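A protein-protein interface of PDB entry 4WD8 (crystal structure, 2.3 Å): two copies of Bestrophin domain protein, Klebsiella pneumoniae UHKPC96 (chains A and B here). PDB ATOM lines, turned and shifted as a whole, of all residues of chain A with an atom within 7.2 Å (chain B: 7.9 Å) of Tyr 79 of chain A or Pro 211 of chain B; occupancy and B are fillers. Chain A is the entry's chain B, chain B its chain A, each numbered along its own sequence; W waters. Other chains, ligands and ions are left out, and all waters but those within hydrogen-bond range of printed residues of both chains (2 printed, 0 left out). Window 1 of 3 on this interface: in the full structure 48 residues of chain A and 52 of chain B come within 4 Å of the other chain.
The side-chain hydroxyl of Tyr 214 of chain B is in hydrogen-bond range of the side-chain amide oxygen of Asn 75 of chain A (2.5 Å).
The backbone carbonyl oxygen of Ser 76 of chain A is in hydrogen-bond range of the side-chain hydroxyl of Ser 80 of chain A (3.2 Å).
Phe 73 of chain B touches Phe 73 of chain A. CE1 of Phe 73 of chain B touches CB of Ser 76 of chain A, 3.6 Å away. Ala 77 of chain B touches Tyr 79 of chain A (CB to CE2, 3.6 Å). Tyr 79 of chain A touches Pro 211 of chain B (CE1 to CD, 3.7 Å). Tyr 79 of chain A touches Tyr 214 of chain B (CB to OH, 3.6 Å). Tyr 214 of chain B touches Leu 258 of chain A. Leu 262 of chain A touches Tyr 214 of chain B (CD1 to OH, 3.1 Å). CB of Ala 213 of chain B touches ND2 of Asn 271 of chain A (3.5 Å).
Printed residues of chain B within 4 Å of Ser 76 of chain A: Phe 73. Of chain B, only Ala 77, Pro 211 and Tyr 214 come within 4 Å of Tyr 79 of chain A. Of the printed residues of chain B, Asn 271 of chain A touches Ala 213 (3.5 Å). Arg 81 of chain B touches none of the printed residues of chain A. Pro 211 of chain B touches just one residue of chain A: Tyr 79 (3.7 Å). Of the printed residues of chain A, Ala 213 of chain B touches Asn 271. Of the printed residues of chain A, Tyr 214 of chain B touches Asn 75, Tyr 79, Leu 258 and Leu 262. Thr 215 of chain B touches none of the printed residues of chain A. The nearest printed residue of chain A that does not touch Pro 211 of chain B is Leu 262 of chain A (4.4 Å). The nearest printed residue of chain B that does not touch Asn 271 of chain A is Pro 211 of chain B (4.8 Å).
Printed residues of chain B that touch a printed residue of chain A: Phe 73, Ala 77, Pro 211, Ala 213 and Tyr 214. Hydrophobic or aromatic side chains of chain B within 4 Å of the printed part of chain A: Phe 73, Ala 77, Pro 211, Ala 213 and Tyr 214. Of the 18 printed residues of chain A, 7 touch a printed residue of chain B. Among the printed residues, 9 pairs touch across the chains. Among the printed residues, no Asp or Glu carboxylate lies within 4 Å of a Lys or Arg side-chain nitrogen of the other chain.
Phe 73 of chain A touches its own counterpart, Phe 73 of chain B. Ser 76 of chain A touches Phe 73 of chain B, but with the chains exchanged Phe 73 of chain A does not touch Ser 76 of chain B (10.1 Å).
Water W1 bridges the side-chain hydroxyl of Tyr 79 of chain A (2.6 Å) and the backbone carbonyl oxygen of Ala 77 of chain B (2.8 Å). Water W2 bridges OH of Tyr 79 of chain A (2.9 Å) and O of Pro 209 of chain B (3.1 Å).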
ATOM      1  N   PHE A  73      17.764   7.676  17.751  1.00  0.00           N
ATOM      2  CA  PHE A  73      18.256   6.535  18.510  1.00  0.00           C
ATOM      3  C   PHE A  73      17.746   5.205  17.961  1.00  0.00           C
ATOM      4  O   PHE A  73      18.499   4.234  17.886  1.00  0.00           O
ATOM      5  CB  PHE A  73      17.881   6.664  19.989  1.00  0.00           C
ATOM      6  CG  PHE A  73      18.801   7.561  20.775  1.00  0.00           C
ATOM      7  CD1 PHE A  73      20.063   7.117  21.165  1.00  0.00           C
ATOM      8  CD2 PHE A  73      18.401   8.843  21.134  1.00  0.00           C
ATOM      9  CE1 PHE A  73      20.908   7.940  21.896  1.00  0.00           C
ATOM     10  CE2 PHE A  73      19.239   9.669  21.865  1.00  0.00           C
ATOM     11  CZ  PHE A  73      20.491   9.225  22.244  1.00  0.00           C
ATOM     12  N   ARG A  74      16.477   5.168  17.560  1.00  0.00           N
ATOM     13  CA  ARG A  74      15.878   3.939  17.054  1.00  0.00           C
ATOM     14  C   ARG A  74      16.599   3.489  15.788  1.00  0.00           C
ATOM     15  O   ARG A  74      16.959   2.318  15.648  1.00  0.00           O
ATOM     16  CB  ARG A  74      14.376   4.127  16.787  1.00  0.00           C
ATOM     17  CG  ARG A  74      13.525   2.862  16.967  1.00  0.00           C
ATOM     18  CD  ARG A  74      13.748   1.832  15.866  1.00  0.00           C
ATOM     19  NE  ARG A  74      12.676   1.801  14.871  1.00  0.00           N
ATOM     20  CZ  ARG A  74      11.744   0.851  14.794  1.00  0.00           C
ATOM     21  NH1 ARG A  74      11.740  -0.159  15.654  1.00  0.00           N
ATOM     22  NH2 ARG A  74      10.815   0.906  13.849  1.00  0.00           N
ATOM     23  N   ASN A  75      16.795   4.425  14.866  1.00  0.00           N
ATOM     24  CA  ASN A  75      17.462   4.136  13.606  1.00  0.00           C
ATOM     25  C   ASN A  75      18.907   3.690  13.839  1.00  0.00           C
ATOM     26  O   ASN A  75      19.400   2.765  13.190  1.00  0.00           O
ATOM     27  CB  ASN A  75      17.368   5.369  12.693  1.00  0.00           C
ATOM     28  CG  ASN A  75      17.753   5.074  11.260  1.00  0.00           C
ATOM     29  OD1 ASN A  75      18.858   4.610  10.980  1.00  0.00           O
ATOM     30  ND2 ASN A  75      16.816   5.288  10.347  1.00  0.00           N
ATOM     31  N   SER A  76      19.562   4.312  14.810  1.00  0.00           N
ATOM     32  CA  SER A  76      20.911   3.915  15.197  1.00  0.00           C
ATOM     33  C   SER A  76      20.949   2.462  15.678  1.00  0.00           C
ATOM     34  O   SER A  76      21.849   1.701  15.314  1.00  0.00           O
ATOM     35  CB  SER A  76      21.434   4.842  16.289  1.00  0.00           C
ATOM     36  OG  SER A  76      22.784   4.550  16.599  1.00  0.00           O
ATOM     37  N   ALA A  77      19.973   2.077  16.498  1.00  0.00           N
ATOM     38  CA  ALA A  77      19.877   0.693  16.955  1.00  0.00           C
ATOM     39  C   ALA A  77      19.597  -0.269  15.787  1.00  0.00           C
ATOM     40  O   ALA A  77      20.155  -1.363  15.731  1.00  0.00           O
ATOM     41  CB  ALA A  77      18.808   0.556  18.047  1.00  0.00           C
ATOM     42  N   SER A  78      18.749   0.142  14.848  1.00  0.00           N
ATOM     43  CA  SER A  78      18.455  -0.698  13.689  1.00  0.00           C
ATOM     44  C   SER A  78      19.690  -0.898  12.808  1.00  0.00           C
ATOM     45  O   SER A  78      19.949  -2.004  12.334  1.00  0.00           O
ATOM     46  CB  SER A  78      17.331  -0.089  12.848  1.00  0.00           C
ATOM     47  OG  SER A  78      16.190   0.176  13.638  1.00  0.00           O
ATOM     48  N   TYR A  79      20.441   0.175  12.579  1.00  0.00           N
ATOM     49  CA  TYR A  79      21.642   0.096  11.755  1.00  0.00           C
ATOM     50  C   TYR A  79      22.676  -0.836  12.391  1.00  0.00           C
ATOM     51  O   TYR A  79      23.345  -1.591  11.686  1.00  0.00           O
ATOM     52  CB  TYR A  79      22.228   1.488  11.491  1.00  0.00           C
ATOM     53  CG  TYR A  79      23.495   1.453  10.662  1.00  0.00           C
ATOM     54  CD1 TYR A  79      23.440   1.166   9.303  1.00  0.00           C
ATOM     55  CD2 TYR A  79      24.734   1.752  11.220  1.00  0.00           C
ATOM     56  CE1 TYR A  79      24.582   1.134   8.530  1.00  0.00           C
ATOM     57  CE2 TYR A  79      25.888   1.732  10.449  1.00  0.00           C
ATOM     58  CZ  TYR A  79      25.803   1.423   9.102  1.00  0.00           C
ATOM     59  OH  TYR A  79      26.938   1.389   8.315  1.00  0.00           O
ATOM     60  N   SER A  80      22.808  -0.781  13.715  1.00  0.00           N
ATOM     61  CA  SER A  80      23.740  -1.665  14.421  1.00  0.00           C
ATOM     62  C   SER A  80      23.410  -3.144  14.196  1.00  0.00           C
ATOM     63  O   SER A  80      24.314  -3.959  14.044  1.00  0.00           O
ATOM     64  CB  SER A  80      23.745  -1.373  15.933  1.00  0.00           C
ATOM     65  OG  SER A  80      24.371  -0.138  16.214  1.00  0.00           O
ATOM     66  N   ARG A  81      22.124  -3.486  14.152  1.00  0.00           N
ATOM     67  CA  ARG A  81      21.719  -4.872  13.916  1.00  0.00           C
ATOM     68  C   ARG A  81      22.108  -5.283  12.507  1.00  0.00           C
ATOM     69  O   ARG A  81      22.577  -6.401  12.281  1.00  0.00           O
ATOM     70  CB  ARG A  81      20.216  -5.063  14.123  1.00  0.00           C
ATOM     71  CG  ARG A  81      19.795  -5.054  15.569  1.00  0.00           C
ATOM     72  CD  ARG A  81      18.280  -5.016  15.708  1.00  0.00           C
ATOM     73  NE  ARG A  81      17.612  -6.065  14.936  1.00  0.00           N
ATOM     74  CZ  ARG A  81      17.425  -7.310  15.364  1.00  0.00           C
ATOM     75  NH1 ARG A  81      17.852  -7.674  16.568  1.00  0.00           N
ATOM     76  NH2 ARG A  81      16.803  -8.191  14.591  1.00  0.00           N
ATOM     77  N   PHE A  82      21.919  -4.358  11.571  1.00  0.00           N
ATOM     78  CA  PHE A  82      22.315  -4.563  10.186  1.00  0.00           C
ATOM     79  C   PHE A  82      23.807  -4.801  10.073  1.00  0.00           C
ATOM     80  O   PHE A  82      24.249  -5.729   9.404  1.00  0.00           O
ATOM     81  CB  PHE A  82      21.940  -3.328   9.353  1.00  0.00           C
ATOM     82  CG  PHE A  82      22.312  -3.432   7.895  1.00  0.00           C
ATOM     83  CD1 PHE A  82      21.425  -3.961   6.966  1.00  0.00           C
ATOM     84  CD2 PHE A  82      23.551  -2.983   7.453  1.00  0.00           C
ATOM     85  CE1 PHE A  82      21.769  -4.039   5.627  1.00  0.00           C
ATOM     86  CE2 PHE A  82      23.904  -3.067   6.116  1.00  0.00           C
ATOM     87  CZ  PHE A  82      23.012  -3.596   5.201  1.00  0.00           C
ATOM     88  N   VAL A  83      24.582  -3.957  10.740  1.00  0.00           N
ATOM     89  CA  VAL A  83      26.031  -4.063  10.695  1.00  0.00           C
ATOM     90  C   VAL A  83      26.513  -5.373  11.315  1.00  0.00           C
ATOM     91  O   VAL A  83      27.354  -6.050  10.738  1.00  0.00           O
ATOM     92  CB  VAL A  83      26.685  -2.839  11.366  1.00  0.00           C
ATOM     93  CG1 VAL A  83      28.127  -3.115  11.749  1.00  0.00           C
ATOM     94  CG2 VAL A  83      26.575  -1.636  10.434  1.00  0.00           C
ATOM     95  N   GLU A  84      25.947  -5.761  12.455  1.00  0.00           N
ATOM     96  CA  GLU A  84      26.344  -7.031  13.056  1.00  0.00           C
ATOM     97  C   GLU A  84      26.030  -8.220  12.154  1.00  0.00           C
ATOM     98  O   GLU A  84      26.851  -9.121  12.002  1.00  0.00           O
ATOM     99  CB  GLU A  84      25.718  -7.248  14.431  1.00  0.00           C
ATOM    100  CG  GLU A  84      26.401  -8.396  15.164  1.00  0.00           C
ATOM    101  CD  GLU A  84      25.672  -8.850  16.409  1.00  0.00           C
ATOM    102  OE1 GLU A  84      24.641  -8.235  16.769  1.00  0.00           O
ATOM    103  OE2 GLU A  84      26.139  -9.835  17.025  1.00  0.00           O
ATOM    104  N   ALA A  85      24.846  -8.202  11.549  1.00  0.00           N
ATOM    105  CA  ALA A  85      24.432  -9.241  10.611  1.00  0.00           C
ATOM    106  C   ALA A  85      25.383  -9.377   9.429  1.00  0.00           C
ATOM    107  O   ALA A  85      25.724 -10.492   9.022  1.00  0.00           O
ATOM    108  CB  ALA A  85      23.007  -8.980  10.116  1.00  0.00           C
ATOM    109  N   LEU A 258      12.900   3.392   7.051  1.00  0.00           N
ATOM    110  CA  LEU A 258      14.238   2.856   6.838  1.00  0.00           C
ATOM    111  C   LEU A 258      14.703   2.067   8.070  1.00  0.00           C
ATOM    112  O   LEU A 258      15.325   1.013   7.951  1.00  0.00           O
ATOM    113  CB  LEU A 258      15.219   3.975   6.500  1.00  0.00           C
ATOM    114  CG  LEU A 258      16.671   3.536   6.343  1.00  0.00           C
ATOM    115  CD1 LEU A 258      16.792   2.475   5.253  1.00  0.00           C
ATOM    116  CD2 LEU A 258      17.537   4.732   6.025  1.00  0.00           C
ATOM    117  N   ALA A 259      14.395   2.586   9.255  1.00  0.00           N
ATOM    118  CA  ALA A 259      14.723   1.888  10.495  1.00  0.00           C
ATOM    119  C   ALA A 259      13.985   0.556  10.548  1.00  0.00           C
ATOM    120  O   ALA A 259      14.537  -0.450  10.982  1.00  0.00           O
ATOM    121  CB  ALA A 259      14.358   2.739  11.693  1.00  0.00           C
ATOM    122  N   LEU A 262      15.870  -1.944   8.227  1.00  0.00           N
ATOM    123  CA  LEU A 262      17.183  -2.410   8.682  1.00  0.00           C
ATOM    124  C   LEU A 262      17.113  -3.342   9.887  1.00  0.00           C
ATOM    125  O   LEU A 262      18.051  -4.097  10.137  1.00  0.00           O
ATOM    126  CB  LEU A 262      18.103  -1.230   9.002  1.00  0.00           C
ATOM    127  CG  LEU A 262      18.529  -0.393   7.795  1.00  0.00           C
ATOM    128  CD1 LEU A 262      19.377   0.768   8.254  1.00  0.00           C
ATOM    129  CD2 LEU A 262      19.285  -1.235   6.780  1.00  0.00           C
ATOM    130  N   GLU A 263      16.006  -3.292  10.624  1.00  0.00           N
ATOM    131  CA  GLU A 263      15.845  -4.090  11.840  1.00  0.00           C
ATOM    132  C   GLU A 263      15.707  -5.558  11.521  1.00  0.00           C
ATOM    133  O   GLU A 263      15.899  -6.411  12.383  1.00  0.00           O
ATOM    134  CB  GLU A 263      14.618  -3.652  12.617  1.00  0.00           C
ATOM    135  CG  GLU A 263      14.896  -2.603  13.619  1.00  0.00           C
ATOM    136  CD  GLU A 263      13.638  -1.973  14.133  1.00  0.00           C
ATOM    137  OE1 GLU A 263      12.538  -2.382  13.699  1.00  0.00           O
ATOM    138  OE2 GLU A 263      13.752  -1.108  15.019  1.00  0.00           O
ATOM    139  N   ASN A 271      16.817  -2.607   1.206  1.00  0.00           N
ATOM    140  CA  ASN A 271      17.917  -2.187   2.057  1.00  0.00           C
ATOM    141  C   ASN A 271      18.403  -3.302   2.976  1.00  0.00           C
ATOM    142  O   ASN A 271      19.186  -3.055   3.888  1.00  0.00           O
ATOM    143  CB  ASN A 271      17.514  -0.949   2.851  1.00  0.00           C
ATOM    144  CG  ASN A 271      17.300   0.257   1.963  1.00  0.00           C
ATOM    145  OD1 ASN A 271      17.943   0.396   0.927  1.00  0.00           O
ATOM    146  ND2 ASN A 271      16.353   1.104   2.334  1.00  0.00           N
ATOM    147  N   PHE B  73      23.754  11.137  13.059  1.00  0.00           N
ATOM    148  CA  PHE B  73      23.798   9.681  13.111  1.00  0.00           C
ATOM    149  C   PHE B  73      24.405   9.098  11.838  1.00  0.00           C
ATOM    150  O   PHE B  73      25.161   8.132  11.885  1.00  0.00           O
ATOM    151  CB  PHE B  73      22.406   9.091  13.387  1.00  0.00           C
ATOM    152  CG  PHE B  73      22.013   9.129  14.847  1.00  0.00           C
ATOM    153  CD1 PHE B  73      22.579   8.239  15.759  1.00  0.00           C
ATOM    154  CD2 PHE B  73      21.075  10.043  15.310  1.00  0.00           C
ATOM    155  CE1 PHE B  73      22.230   8.275  17.105  1.00  0.00           C
ATOM    156  CE2 PHE B  73      20.715  10.081  16.655  1.00  0.00           C
ATOM    157  CZ  PHE B  73      21.292   9.196  17.551  1.00  0.00           C
ATOM    158  N   ARG B  74      24.071   9.687  10.698  1.00  0.00           N
ATOM    159  CA  ARG B  74      24.604   9.215   9.430  1.00  0.00           C
ATOM    160  C   ARG B  74      26.116   9.391   9.326  1.00  0.00           C
ATOM    161  O   ARG B  74      26.824   8.459   8.945  1.00  0.00           O
ATOM    162  CB  ARG B  74      23.902   9.923   8.274  1.00  0.00           C
ATOM    163  CG  ARG B  74      24.067   9.268   6.906  1.00  0.00           C
ATOM    164  CD  ARG B  74      25.384   9.668   6.273  1.00  0.00           C
ATOM    165  NE  ARG B  74      25.445  11.120   6.143  1.00  0.00           N
ATOM    166  CZ  ARG B  74      25.147  11.791   5.038  1.00  0.00           C
ATOM    167  NH1 ARG B  74      24.746  11.144   3.954  1.00  0.00           N
ATOM    168  NH2 ARG B  74      25.230  13.114   5.027  1.00  0.00           N
ATOM    169  N   SER B  76      28.120   9.619  11.602  1.00  0.00           N
ATOM    170  CA  SER B  76      28.638   8.688  12.581  1.00  0.00           C
ATOM    171  C   SER B  76      28.897   7.315  11.930  1.00  0.00           C
ATOM    172  O   SER B  76      29.951   6.713  12.127  1.00  0.00           O
ATOM    173  CB  SER B  76      27.633   8.595  13.734  1.00  0.00           C
ATOM    174  OG  SER B  76      28.128   7.834  14.804  1.00  0.00           O
ATOM    175  N   ALA B  77      27.947   6.836  11.133  1.00  0.00           N
ATOM    176  CA  ALA B  77      28.123   5.574  10.408  1.00  0.00           C
ATOM    177  C   ALA B  77      29.220   5.654   9.341  1.00  0.00           C
ATOM    178  O   ALA B  77      30.000   4.714   9.169  1.00  0.00           O
ATOM    179  CB  ALA B  77      26.808   5.129   9.784  1.00  0.00           C
ATOM    180  N   SER B  78      29.279   6.781   8.636  1.00  0.00           N
ATOM    181  CA  SER B  78      30.274   6.986   7.589  1.00  0.00           C
ATOM    182  C   SER B  78      31.658   6.997   8.209  1.00  0.00           C
ATOM    183  O   SER B  78      32.610   6.439   7.665  1.00  0.00           O
ATOM    184  CB  SER B  78      30.024   8.296   6.851  1.00  0.00           C
ATOM    185  OG  SER B  78      28.690   8.362   6.384  1.00  0.00           O
ATOM    186  N   SER B  80      32.621   5.586  11.160  1.00  0.00           N
ATOM    187  CA  SER B  80      32.994   4.265  11.660  1.00  0.00           C
ATOM    188  C   SER B  80      33.507   3.358  10.552  1.00  0.00           C
ATOM    189  O   SER B  80      34.434   2.574  10.752  1.00  0.00           O
ATOM    190  CB  SER B  80      31.810   3.600  12.356  1.00  0.00           C
ATOM    191  OG  SER B  80      31.529   4.249  13.577  1.00  0.00           O
ATOM    192  N   ARG B  81      32.892   3.477   9.381  1.00  0.00           N
ATOM    193  CA  ARG B  81      33.274   2.687   8.225  1.00  0.00           C
ATOM    194  C   ARG B  81      34.666   3.059   7.718  1.00  0.00           C
ATOM    195  O   ARG B  81      35.456   2.187   7.347  1.00  0.00           O
ATOM    196  CB  ARG B  81      32.221   2.862   7.118  1.00  0.00           C
ATOM    197  CG  ARG B  81      32.593   2.286   5.761  1.00  0.00           C
ATOM    198  CD  ARG B  81      31.477   2.534   4.750  1.00  0.00           C
ATOM    199  NE  ARG B  81      31.985   2.546   3.378  1.00  0.00           N
ATOM    200  CZ  ARG B  81      31.995   1.478   2.598  1.00  0.00           C
ATOM    201  NH1 ARG B  81      31.523   0.335   3.073  1.00  0.00           N
ATOM    202  NH2 ARG B  81      32.477   1.545   1.363  1.00  0.00           N
ATOM    203  N   LEU B 205      33.640  -4.267   3.155  1.00  0.00           N
ATOM    204  CA  LEU B 205      33.476  -2.812   3.095  1.00  0.00           C
ATOM    205  C   LEU B 205      33.332  -2.293   1.666  1.00  0.00           C
ATOM    206  O   LEU B 205      32.607  -1.333   1.427  1.00  0.00           O
ATOM    207  CB  LEU B 205      34.637  -2.084   3.777  1.00  0.00           C
ATOM    208  CG  LEU B 205      34.755  -2.133   5.300  1.00  0.00           C
ATOM    209  CD1 LEU B 205      35.962  -1.328   5.750  1.00  0.00           C
ATOM    210  CD2 LEU B 205      33.487  -1.620   5.972  1.00  0.00           C
ATOM    211  N   THR B 208      29.694  -3.652   0.635  1.00  0.00           N
ATOM    212  CA  THR B 208      28.712  -3.009   1.516  1.00  0.00           C
ATOM    213  C   THR B 208      28.989  -1.536   1.840  1.00  0.00           C
ATOM    214  O   THR B 208      29.797  -1.238   2.718  1.00  0.00           O
ATOM    215  CB  THR B 208      28.627  -3.779   2.859  1.00  0.00           C
ATOM    216  OG1 THR B 208      28.547  -5.189   2.607  1.00  0.00           O
ATOM    217  CG2 THR B 208      27.438  -3.309   3.694  1.00  0.00           C
ATOM    218  N   PRO B 209      28.252  -0.613   1.214  1.00  0.00           N
ATOM    219  CA  PRO B 209      28.321   0.791   1.622  1.00  0.00           C
ATOM    220  C   PRO B 209      27.356   1.082   2.768  1.00  0.00           C
ATOM    221  O   PRO B 209      26.525   0.235   3.095  1.00  0.00           O
ATOM    222  CB  PRO B 209      27.884   1.541   0.363  1.00  0.00           C
ATOM    223  CG  PRO B 209      26.970   0.601  -0.328  1.00  0.00           C
ATOM    224  CD  PRO B 209      27.393  -0.803   0.033  1.00  0.00           C
ATOM    225  N   VAL B 210      27.508   2.233   3.412  1.00  0.00           N
ATOM    226  CA  VAL B 210      26.405   2.793   4.171  1.00  0.00           C
ATOM    227  C   VAL B 210      25.237   2.786   3.187  1.00  0.00           C
ATOM    228  O   VAL B 210      25.374   3.287   2.069  1.00  0.00           O
ATOM    229  CB  VAL B 210      26.712   4.220   4.626  1.00  0.00           C
ATOM    230  CG1 VAL B 210      25.501   4.834   5.328  1.00  0.00           C
ATOM    231  CG2 VAL B 210      27.930   4.214   5.552  1.00  0.00           C
ATOM    232  N   PRO B 211      24.085   2.225   3.596  1.00  0.00           N
ATOM    233  CA  PRO B 211      22.980   2.012   2.648  1.00  0.00           C
ATOM    234  C   PRO B 211      22.563   3.284   1.916  1.00  0.00           C
ATOM    235  O   PRO B 211      22.554   4.374   2.481  1.00  0.00           O
ATOM    236  CB  PRO B 211      21.842   1.522   3.548  1.00  0.00           C
ATOM    237  CG  PRO B 211      22.542   0.873   4.706  1.00  0.00           C
ATOM    238  CD  PRO B 211      23.800   1.663   4.929  1.00  0.00           C
ATOM    239  N   PHE B 212      22.228   3.125   0.642  1.00  0.00           N
ATOM    240  CA  PHE B 212      22.033   4.264  -0.239  1.00  0.00           C
ATOM    241  C   PHE B 212      20.808   5.074   0.114  1.00  0.00           C
ATOM    242  O   PHE B 212      20.711   6.249  -0.238  1.00  0.00           O
ATOM    243  CB  PHE B 212      21.900   3.769  -1.683  1.00  0.00           C
ATOM    244  CG  PHE B 212      21.758   4.872  -2.693  1.00  0.00           C
ATOM    245  CD1 PHE B 212      22.624   5.954  -2.694  1.00  0.00           C
ATOM    246  CD2 PHE B 212      20.735   4.841  -3.625  1.00  0.00           C
ATOM    247  CE1 PHE B 212      22.481   6.972  -3.619  1.00  0.00           C
ATOM    248  CE2 PHE B 212      20.587   5.855  -4.552  1.00  0.00           C
ATOM    249  CZ  PHE B 212      21.461   6.922  -4.548  1.00  0.00           C
ATOM    250  N   ALA B 213      19.898   4.489   0.877  1.00  0.00           N
ATOM    251  CA  ALA B 213      18.689   5.225   1.178  1.00  0.00           C
ATOM    252  C   ALA B 213      18.950   6.247   2.260  1.00  0.00           C
ATOM    253  O   ALA B 213      18.163   7.167   2.433  1.00  0.00           O
ATOM    254  CB  ALA B 213      17.569   4.276   1.589  1.00  0.00           C
ATOM    255  N   TYR B 214      20.095   6.143   2.929  1.00  0.00           N
ATOM    256  CA  TYR B 214      20.458   7.161   3.901  1.00  0.00           C
ATOM    257  C   TYR B 214      20.886   8.424   3.176  1.00  0.00           C
ATOM    258  O   TYR B 214      20.439   9.525   3.487  1.00  0.00           O
ATOM    259  CB  TYR B 214      21.620   6.692   4.768  1.00  0.00           C
ATOM    260  CG  TYR B 214      21.233   5.866   5.964  1.00  0.00           C
ATOM    261  CD1 TYR B 214      20.475   6.397   6.995  1.00  0.00           C
ATOM    262  CD2 TYR B 214      21.674   4.557   6.080  1.00  0.00           C
ATOM    263  CE1 TYR B 214      20.139   5.631   8.096  1.00  0.00           C
ATOM    264  CE2 TYR B 214      21.354   3.787   7.173  1.00  0.00           C
ATOM    265  CZ  TYR B 214      20.588   4.322   8.175  1.00  0.00           C
ATOM    266  OH  TYR B 214      20.275   3.537   9.255  1.00  0.00           O
ATOM    267  N   THR B 215      21.712   8.231   2.154  1.00  0.00           N
ATOM    268  CA  THR B 215      22.224   9.329   1.354  1.00  0.00           C
ATOM    269  C   THR B 215      21.130   9.980   0.525  1.00  0.00           C
ATOM    270  O   THR B 215      21.050  11.201   0.443  1.00  0.00           O
ATOM    271  CB  THR B 215      23.407   8.877   0.460  1.00  0.00           C
ATOM    272  OG1 THR B 215      24.510   8.490   1.289  1.00  0.00           O
ATOM    273  CG2 THR B 215      23.847  10.000  -0.466  1.00  0.00           C
ATOM    274  N   LEU B 216      20.261   9.157  -0.050  1.00  0.00           N
ATOM    275  CA  LEU B 216      19.169   9.650  -0.878  1.00  0.00           C
ATOM    276  C   LEU B 216      18.226  10.548  -0.082  1.00  0.00           C
ATOM    277  O   LEU B 216      17.934  11.671  -0.492  1.00  0.00           O
ATOM    278  CB  LEU B 216      18.403   8.472  -1.480  1.00  0.00           C
ATOM    279  CG  LEU B 216      17.217   8.811  -2.375  1.00  0.00           C
ATOM    280  CD1 LEU B 216      17.728   9.533  -3.610  1.00  0.00           C
ATOM    281  CD2 LEU B 216      16.470   7.541  -2.767  1.00  0.00           C
ATOM    282  N   ILE B 217      17.751  10.045   1.055  1.00  0.00           N
ATOM    283  CA  ILE B 217      16.939  10.828   1.973  1.00  0.00           C
ATOM    284  C   ILE B 217      17.642  12.134   2.333  1.00  0.00           C
ATOM    285  O   ILE B 217      17.093  13.219   2.133  1.00  0.00           O
ATOM    286  CB  ILE B 217      16.621  10.048   3.265  1.00  0.00           C
ATOM    287  CG1 ILE B 217      15.671   8.887   2.969  1.00  0.00           C
ATOM    288  CG2 ILE B 217      16.011  10.969   4.314  1.00  0.00           C
ATOM    289  CD1 ILE B 217      15.533   7.915   4.123  1.00  0.00           C
ATOM    290  N   GLU B 263      33.190   8.297   2.849  1.00  0.00           N
ATOM    291  CA  GLU B 263      32.540   7.102   2.296  1.00  0.00           C
ATOM    292  C   GLU B 263      33.314   6.264   1.261  1.00  0.00           C
ATOM    293  O   GLU B 263      32.895   5.155   0.932  1.00  0.00           O
ATOM    294  CB  GLU B 263      31.168   7.498   1.755  1.00  0.00           C
ATOM    295  CG  GLU B 263      30.112   7.373   2.862  1.00  0.00           C
ATOM    296  CD  GLU B 263      28.805   8.080   2.559  1.00  0.00           C
ATOM    297  OE1 GLU B 263      28.672   8.665   1.460  1.00  0.00           O
ATOM    298  OE2 GLU B 263      27.918   8.068   3.441  1.00  0.00           O
HETATM  299  O   HOH W   1      29.057   2.075   9.566  1.00  0.00           O
HETATM  300  O   HOH W   2      27.001  -0.430   6.080  1.00  0.00           O
